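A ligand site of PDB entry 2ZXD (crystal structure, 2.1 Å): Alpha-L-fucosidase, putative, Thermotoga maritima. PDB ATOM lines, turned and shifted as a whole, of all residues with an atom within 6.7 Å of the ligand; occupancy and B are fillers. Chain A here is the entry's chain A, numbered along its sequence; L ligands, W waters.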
ATOM      1  N   PHE A  32      10.833 -19.934  10.005  1.00  0.00           N
ATOM      2  CA  PHE A  32       9.924 -19.018  10.646  1.00  0.00           C
ATOM      3  C   PHE A  32       9.792 -17.831   9.638  1.00  0.00           C
ATOM      4  O   PHE A  32      10.758 -17.499   8.922  1.00  0.00           O
ATOM      5  CB  PHE A  32      10.655 -18.482  11.909  1.00  0.00           C
ATOM      6  CG  PHE A  32       9.816 -18.391  13.160  1.00  0.00           C
ATOM      7  CD1 PHE A  32       8.428 -18.491  13.098  1.00  0.00           C
ATOM      8  CD2 PHE A  32      10.450 -18.266  14.424  1.00  0.00           C
ATOM      9  CE1 PHE A  32       7.634 -18.459  14.308  1.00  0.00           C
ATOM     10  CE2 PHE A  32       9.721 -18.238  15.607  1.00  0.00           C
ATOM     11  CZ  PHE A  32       8.299 -18.341  15.569  1.00  0.00           C
ATOM     12  N   HIS A  34       8.558 -13.814   9.836  1.00  0.00           N
ATOM     13  CA  HIS A  34       7.885 -12.643  10.415  1.00  0.00           C
ATOM     14  C   HIS A  34       7.639 -11.723   9.244  1.00  0.00           C
ATOM     15  O   HIS A  34       8.583 -11.136   8.651  1.00  0.00           O
ATOM     16  CB  HIS A  34       8.698 -11.956  11.516  1.00  0.00           C
ATOM     17  CG  HIS A  34       8.718 -12.726  12.828  1.00  0.00           C
ATOM     18  ND1 HIS A  34       9.148 -14.045  12.906  1.00  0.00           N
ATOM     19  CD2 HIS A  34       8.363 -12.373  14.085  1.00  0.00           C
ATOM     20  CE1 HIS A  34       9.066 -14.462  14.162  1.00  0.00           C
ATOM     21  NE2 HIS A  34       8.592 -13.468  14.901  1.00  0.00           N
ATOM     22  N   TYR A  64      14.520  -5.100  16.823  1.00  0.00           N
ATOM     23  CA  TYR A  64      13.481  -5.872  16.151  1.00  0.00           C
ATOM     24  C   TYR A  64      12.564  -4.972  15.326  1.00  0.00           C
ATOM     25  O   TYR A  64      11.760  -4.235  15.880  1.00  0.00           O
ATOM     26  CB  TYR A  64      12.619  -6.634  17.172  1.00  0.00           C
ATOM     27  CG  TYR A  64      13.305  -7.778  17.917  1.00  0.00           C
ATOM     28  CD1 TYR A  64      14.615  -8.167  17.620  1.00  0.00           C
ATOM     29  CD2 TYR A  64      12.596  -8.496  18.905  1.00  0.00           C
ATOM     30  CE1 TYR A  64      15.228  -9.242  18.287  1.00  0.00           C
ATOM     31  CE2 TYR A  64      13.189  -9.578  19.576  1.00  0.00           C
ATOM     32  CZ  TYR A  64      14.509  -9.945  19.251  1.00  0.00           C
ATOM     33  OH  TYR A  64      15.076 -11.003  19.909  1.00  0.00           O
ATOM     34  N   GLU A  66      10.024  -5.660  13.702  1.00  0.00           N
ATOM     35  CA  GLU A  66       8.614  -5.961  13.848  1.00  0.00           C
ATOM     36  C   GLU A  66       8.002  -5.223  15.041  1.00  0.00           C
ATOM     37  O   GLU A  66       6.792  -5.182  15.178  1.00  0.00           O
ATOM     38  CB  GLU A  66       8.341  -7.479  13.932  1.00  0.00           C
ATOM     39  CG  GLU A  66       8.763  -8.188  15.211  1.00  0.00           C
ATOM     40  CD  GLU A  66      10.264  -8.490  15.308  1.00  0.00           C
ATOM     41  OE1 GLU A  66      11.040  -8.052  14.410  1.00  0.00           O
ATOM     42  OE2 GLU A  66      10.661  -9.160  16.314  1.00  0.00           O
ATOM     43  N   TRP A  67       8.834  -4.622  15.887  1.00  0.00           N
ATOM     44  CA  TRP A  67       8.342  -3.855  17.026  1.00  0.00           C
ATOM     45  C   TRP A  67       8.220  -2.363  16.625  1.00  0.00           C
ATOM     46  O   TRP A  67       8.076  -1.481  17.465  1.00  0.00           O
ATOM     47  CB  TRP A  67       9.305  -4.013  18.203  1.00  0.00           C
ATOM     48  CG  TRP A  67       9.035  -5.217  19.111  1.00  0.00           C
ATOM     49  CD1 TRP A  67       9.163  -6.531  18.781  1.00  0.00           C
ATOM     50  CD2 TRP A  67       8.515  -5.174  20.455  1.00  0.00           C
ATOM     51  NE1 TRP A  67       8.735  -7.316  19.828  1.00  0.00           N
ATOM     52  CE2 TRP A  67       8.331  -6.508  20.859  1.00  0.00           C
ATOM     53  CE3 TRP A  67       8.182  -4.129  21.342  1.00  0.00           C
ATOM     54  CZ2 TRP A  67       7.814  -6.853  22.130  1.00  0.00           C
ATOM     55  CZ3 TRP A  67       7.687  -4.444  22.585  1.00  0.00           C
ATOM     56  CH2 TRP A  67       7.497  -5.804  22.977  1.00  0.00           C
ATOM     57  N   THR A 125       3.955 -15.676  10.693  1.00  0.00           N
ATOM     58  CA  THR A 125       3.252 -14.896  11.664  1.00  0.00           C
ATOM     59  C   THR A 125       1.835 -14.625  11.123  1.00  0.00           C
ATOM     60  O   THR A 125       1.710 -13.874  10.159  1.00  0.00           O
ATOM     61  CB  THR A 125       3.973 -13.520  11.862  1.00  0.00           C
ATOM     62  OG1 THR A 125       4.260 -12.913  10.579  1.00  0.00           O
ATOM     63  CG2 THR A 125       5.288 -13.687  12.664  1.00  0.00           C
ATOM     64  N   HIS A 128       0.987 -10.659  14.504  1.00  0.00           N
ATOM     65  CA  HIS A 128       2.054 -10.343  15.457  1.00  0.00           C
ATOM     66  C   HIS A 128       1.509  -9.337  16.489  1.00  0.00           C
ATOM     67  O   HIS A 128       0.298  -9.161  16.609  1.00  0.00           O
ATOM     68  CB  HIS A 128       3.306  -9.813  14.724  1.00  0.00           C
ATOM     69  CG  HIS A 128       4.563  -9.972  15.516  1.00  0.00           C
ATOM     70  ND1 HIS A 128       5.103  -8.947  16.262  1.00  0.00           N
ATOM     71  CD2 HIS A 128       5.362 -11.062  15.722  1.00  0.00           C
ATOM     72  CE1 HIS A 128       6.183  -9.396  16.901  1.00  0.00           C
ATOM     73  NE2 HIS A 128       6.354 -10.672  16.589  1.00  0.00           N
ATOM     74  N   HIS A 129       2.386  -8.710  17.260  1.00  0.00           N
ATOM     75  CA  HIS A 129       1.900  -7.811  18.291  1.00  0.00           C
ATOM     76  C   HIS A 129       1.045  -6.604  17.808  1.00  0.00           C
ATOM     77  O   HIS A 129       0.206  -6.084  18.566  1.00  0.00           O
ATOM     78  CB  HIS A 129       3.079  -7.280  19.121  1.00  0.00           C
ATOM     79  CG  HIS A 129       4.008  -8.348  19.608  1.00  0.00           C
ATOM     80  ND1 HIS A 129       3.606  -9.667  19.775  1.00  0.00           N
ATOM     81  CD2 HIS A 129       5.323  -8.308  19.969  1.00  0.00           C
ATOM     82  CE1 HIS A 129       4.644 -10.373  20.216  1.00  0.00           C
ATOM     83  NE2 HIS A 129       5.689  -9.567  20.328  1.00  0.00           N
ATOM     84  N   TYR A 171       2.031 -19.009  13.622  1.00  0.00           N
ATOM     85  CA  TYR A 171       2.464 -18.233  14.765  1.00  0.00           C
ATOM     86  C   TYR A 171       1.298 -17.265  15.045  1.00  0.00           C
ATOM     87  O   TYR A 171       0.708 -16.706  14.110  1.00  0.00           O
ATOM     88  CB  TYR A 171       3.750 -17.423  14.467  1.00  0.00           C
ATOM     89  CG  TYR A 171       4.049 -16.330  15.482  1.00  0.00           C
ATOM     90  CD1 TYR A 171       5.157 -16.432  16.353  1.00  0.00           C
ATOM     91  CD2 TYR A 171       3.276 -15.172  15.539  1.00  0.00           C
ATOM     92  CE1 TYR A 171       5.477 -15.409  17.220  1.00  0.00           C
ATOM     93  CE2 TYR A 171       3.603 -14.123  16.419  1.00  0.00           C
ATOM     94  CZ  TYR A 171       4.682 -14.253  17.248  1.00  0.00           C
ATOM     95  OH  TYR A 171       4.978 -13.248  18.139  1.00  0.00           O
ATOM     96  N   LEU A 176       0.088 -10.429  23.211  1.00  0.00           N
ATOM     97  CA  LEU A 176       0.152  -9.012  22.976  1.00  0.00           C
ATOM     98  C   LEU A 176      -0.618  -8.658  21.743  1.00  0.00           C
ATOM     99  O   LEU A 176      -0.563  -9.370  20.745  1.00  0.00           O
ATOM    100  CB  LEU A 176       1.629  -8.534  22.762  1.00  0.00           C
ATOM    101  CG  LEU A 176       2.661  -8.521  23.904  1.00  0.00           C
ATOM    102  CD1 LEU A 176       4.005  -7.926  23.407  1.00  0.00           C
ATOM    103  CD2 LEU A 176       2.104  -7.702  25.112  1.00  0.00           C
ATOM    104  N   TRP A 178      -1.385  -4.750  20.272  1.00  0.00           N
ATOM    105  CA  TRP A 178      -1.369  -3.311  20.413  1.00  0.00           C
ATOM    106  C   TRP A 178      -2.652  -2.610  19.904  1.00  0.00           C
ATOM    107  O   TRP A 178      -2.783  -1.404  20.036  1.00  0.00           O
ATOM    108  CB  TRP A 178      -0.080  -2.775  19.717  1.00  0.00           C
ATOM    109  CG  TRP A 178       1.145  -3.298  20.428  1.00  0.00           C
ATOM    110  CD1 TRP A 178       1.240  -3.710  21.741  1.00  0.00           C
ATOM    111  CD2 TRP A 178       2.423  -3.553  19.830  1.00  0.00           C
ATOM    112  NE1 TRP A 178       2.494  -4.210  22.000  1.00  0.00           N
ATOM    113  CE2 TRP A 178       3.257  -4.129  20.857  1.00  0.00           C
ATOM    114  CE3 TRP A 178       2.958  -3.365  18.545  1.00  0.00           C
ATOM    115  CZ2 TRP A 178       4.589  -4.516  20.613  1.00  0.00           C
ATOM    116  CZ3 TRP A 178       4.279  -3.760  18.301  1.00  0.00           C
ATOM    117  CH2 TRP A 178       5.081  -4.331  19.355  1.00  0.00           C
ATOM    118  N   TRP A 222       1.912 -22.209  17.344  1.00  0.00           N
ATOM    119  CA  TRP A 222       3.066 -21.596  17.974  1.00  0.00           C
ATOM    120  C   TRP A 222       2.651 -20.210  18.519  1.00  0.00           C
ATOM    121  O   TRP A 222       2.703 -19.184  17.786  1.00  0.00           O
ATOM    122  CB  TRP A 222       4.145 -21.473  16.881  1.00  0.00           C
ATOM    123  CG  TRP A 222       5.632 -21.494  17.323  1.00  0.00           C
ATOM    124  CD1 TRP A 222       6.528 -22.514  17.104  1.00  0.00           C
ATOM    125  CD2 TRP A 222       6.358 -20.471  18.020  1.00  0.00           C
ATOM    126  NE1 TRP A 222       7.775 -22.182  17.629  1.00  0.00           N
ATOM    127  CE2 TRP A 222       7.690 -20.930  18.200  1.00  0.00           C
ATOM    128  CE3 TRP A 222       6.010 -19.201  18.532  1.00  0.00           C
ATOM    129  CZ2 TRP A 222       8.679 -20.172  18.857  1.00  0.00           C
ATOM    130  CZ3 TRP A 222       7.007 -18.431  19.206  1.00  0.00           C
ATOM    131  CH2 TRP A 222       8.331 -18.938  19.348  1.00  0.00           C
ATOM    132  N   ASP A 224       2.855 -16.902  21.125  1.00  0.00           N
ATOM    133  CA  ASP A 224       3.991 -16.124  21.640  1.00  0.00           C
ATOM    134  C   ASP A 224       3.437 -15.181  22.712  1.00  0.00           C
ATOM    135  O   ASP A 224       2.247 -14.755  22.641  1.00  0.00           O
ATOM    136  CB  ASP A 224       4.634 -15.269  20.526  1.00  0.00           C
ATOM    137  CG  ASP A 224       6.060 -14.836  20.846  1.00  0.00           C
ATOM    138  OD1 ASP A 224       6.647 -14.044  20.048  1.00  0.00           O
ATOM    139  OD2 ASP A 224       6.621 -15.275  21.876  1.00  0.00           O
ATOM    140  N   MET A 225       4.321 -14.876  23.668  1.00  0.00           N
ATOM    141  CA  MET A 225       4.114 -13.933  24.764  1.00  0.00           C
ATOM    142  C   MET A 225       3.078 -14.309  25.813  1.00  0.00           C
ATOM    143  O   MET A 225       2.539 -13.426  26.512  1.00  0.00           O
ATOM    144  CB  MET A 225       3.830 -12.508  24.166  1.00  0.00           C
ATOM    145  CG  MET A 225       4.971 -12.007  23.225  1.00  0.00           C
ATOM    146  SD  MET A 225       6.599 -11.900  24.118  1.00  0.00           S
ATOM    147  CE  MET A 225       6.296 -10.564  25.168  1.00  0.00           C
ATOM    148  N   ARG A 254       4.543 -21.633  24.975  1.00  0.00           N
ATOM    149  CA  ARG A 254       4.425 -20.241  25.373  1.00  0.00           C
ATOM    150  C   ARG A 254       2.996 -19.832  25.692  1.00  0.00           C
ATOM    151  O   ARG A 254       2.594 -18.698  25.419  1.00  0.00           O
ATOM    152  CB  ARG A 254       5.013 -19.369  24.230  1.00  0.00           C
ATOM    153  CG  ARG A 254       6.543 -19.621  24.026  1.00  0.00           C
ATOM    154  CD  ARG A 254       7.145 -18.725  22.941  1.00  0.00           C
ATOM    155  NE  ARG A 254       8.579 -18.940  22.945  1.00  0.00           N
ATOM    156  CZ  ARG A 254       9.455 -17.984  22.660  1.00  0.00           C
ATOM    157  NH1 ARG A 254      10.757 -18.272  22.695  1.00  0.00           N
ATOM    158  NH2 ARG A 254       9.033 -16.757  22.303  1.00  0.00           N
ATOM    159  N   GLU A 266      15.949 -19.664  22.958  1.00  0.00           N
ATOM    160  CA  GLU A 266      16.646 -18.615  22.234  1.00  0.00           C
ATOM    161  C   GLU A 266      17.998 -18.500  22.933  1.00  0.00           C
ATOM    162  O   GLU A 266      18.171 -19.068  23.987  1.00  0.00           O
ATOM    163  CB  GLU A 266      15.883 -17.301  22.319  1.00  0.00           C
ATOM    164  CG  GLU A 266      14.501 -17.424  21.653  1.00  0.00           C
ATOM    165  CD  GLU A 266      13.668 -16.189  21.841  1.00  0.00           C
ATOM    166  OE1 GLU A 266      14.105 -15.100  21.425  1.00  0.00           O
ATOM    167  OE2 GLU A 266      12.580 -16.295  22.419  1.00  0.00           O
ATOM    168  N   THR A 283      15.154 -21.090  18.183  1.00  0.00           N
ATOM    169  CA  THR A 283      14.821 -20.189  17.118  1.00  0.00           C
ATOM    170  C   THR A 283      15.703 -18.924  17.200  1.00  0.00           C
ATOM    171  O   THR A 283      16.103 -18.498  18.281  1.00  0.00           O
ATOM    172  CB  THR A 283      13.307 -19.805  17.161  1.00  0.00           C
ATOM    173  OG1 THR A 283      12.992 -18.940  16.068  1.00  0.00           O
ATOM    174  CG2 THR A 283      12.971 -19.118  18.450  1.00  0.00           C
ATOM    175  N   ARG A 284      16.044 -18.386  16.027  1.00  0.00           N
ATOM    176  CA  ARG A 284      16.748 -17.113  15.887  1.00  0.00           C
ATOM    177  C   ARG A 284      16.608 -16.691  14.414  1.00  0.00           C
ATOM    178  O   ARG A 284      16.181 -17.478  13.545  1.00  0.00           O
ATOM    179  CB  ARG A 284      18.232 -17.186  16.226  1.00  0.00           C
ATOM    180  CG  ARG A 284      19.063 -17.973  15.226  1.00  0.00           C
ATOM    181  CD  ARG A 284      20.507 -17.442  15.290  1.00  0.00           C
ATOM    182  NE  ARG A 284      20.539 -16.082  14.727  1.00  0.00           N
ATOM    183  CZ  ARG A 284      21.519 -15.202  14.934  1.00  0.00           C
ATOM    184  NH1 ARG A 284      22.529 -15.538  15.704  1.00  0.00           N
ATOM    185  NH2 ARG A 284      21.469 -14.007  14.328  1.00  0.00           N
ATOM    186  N   PHE A 290      13.509  -9.938  13.494  1.00  0.00           N
ATOM    187  CA  PHE A 290      12.758 -11.044  12.930  1.00  0.00           C
ATOM    188  C   PHE A 290      12.096 -10.450  11.663  1.00  0.00           C
ATOM    189  O   PHE A 290      12.212 -11.025  10.588  1.00  0.00           O
ATOM    190  CB  PHE A 290      11.759 -11.613  13.934  1.00  0.00           C
ATOM    191  CG  PHE A 290      12.448 -12.465  15.012  1.00  0.00           C
ATOM    192  CD1 PHE A 290      12.967 -11.882  16.177  1.00  0.00           C
ATOM    193  CD2 PHE A 290      12.626 -13.843  14.808  1.00  0.00           C
ATOM    194  CE1 PHE A 290      13.679 -12.674  17.147  1.00  0.00           C
ATOM    195  CE2 PHE A 290      13.321 -14.647  15.765  1.00  0.00           C
ATOM    196  CZ  PHE A 290      13.848 -14.051  16.923  1.00  0.00           C
HETATM  197  C1  LIG L   1      11.288 -15.530  19.057  1.00  0.00           C
HETATM  198  C2  LIG L   1      10.438 -14.589  18.205  1.00  0.00           C
HETATM  199  C3  LIG L   1       9.136 -15.302  17.830  1.00  0.00           C
HETATM  200  C4  LIG L   1      10.166 -13.294  18.973  1.00  0.00           C
HETATM  201  N1  LIG L   1       9.229 -13.542  20.083  1.00  0.00           N
HETATM  202  C5  LIG L   1       9.079 -12.337  20.921  1.00  0.00           C
HETATM  203  C6  LIG L   1       8.474 -11.214  20.059  1.00  0.00           C
HETATM  204  O1  LIG L   1       8.262 -10.039  20.829  1.00  0.00           O
HETATM  205  C7  LIG L   1       9.429 -10.902  18.905  1.00  0.00           C
HETATM  206  O2  LIG L   1       8.892  -9.865  18.088  1.00  0.00           O
HETATM  207  C8  LIG L   1       9.629 -12.178  18.067  1.00  0.00           C
HETATM  208  O3  LIG L   1       8.371 -12.567  17.524  1.00  0.00           O
HETATM  209  O   HOH W   1      10.562  -9.025  22.408  1.00  0.00           O
HETATM  210  O   HOH W   2      10.777 -14.455  22.313  1.00  0.00           O
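O1 of the ligand is in hydrogen-bond range of NE1 of Trp 67 (2.9 Å).
NE2 of His 129 is in hydrogen-bond range of O1 of the ligand.
O3 of the ligand sits at hydrogen-bond distance from NE2 of His 34 (2.8 Å).
NE2 of His 128 lies within hydrogen-bond range of O3 of the ligand (2.9 Å).
OE2 of Glu 66 lies within hydrogen-bond range of O2 of the ligand (2.6 Å).
N1 of the ligand is in salt-bridge range of OD1 of Asp 224 (2.6 Å).
NE2 of His 128 sits close to OH of Tyr 171 (3.3 Å).
OD1 of Asp 224 is in hydrogen-bond range of OH of Tyr 171 (2.7 Å).
OE1 of Glu 66 is in hydrogen-bond range of N of Phe 290 (3.2 Å).
OE2 of Glu 266 is in salt-bridge range of NH1 of Arg 254.
The backbone carbonyl oxygen of His 129 sits at hydrogen-bond distance from the backbone NH of Trp 178.
OD2 of Asp 224 is in salt-bridge range of NH2 of Arg 254, at 2.9 Å.
Phe 32 touches the ligand.
CD2 of Tyr 64 touches C7 of the ligand, at 3.98 Å.
OH of Tyr 171 touches O3 of the ligand, at 3.5 Å.
Arg 254 touches the ligand.
Glu 266 touches the ligand (OE2 to C1, 3.7 Å).
Phe 290 touches the ligand.
Within 4 Å of the ligand: Phe 32, His 34, Tyr 64, Glu 66, Trp 67, His 128, His 129, Tyr 171, Asp 224, Arg 254, Glu 266 and Phe 290.
The nearest printed residue that does not touch the ligand is Thr 283 (4.01 Å).
Water W2 lies within hydrogen-bond range of OE2 of Glu 266 (2.6 Å), N1 of the ligand (2.9 Å) and NH2 of Arg 254 (2.9 Å).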
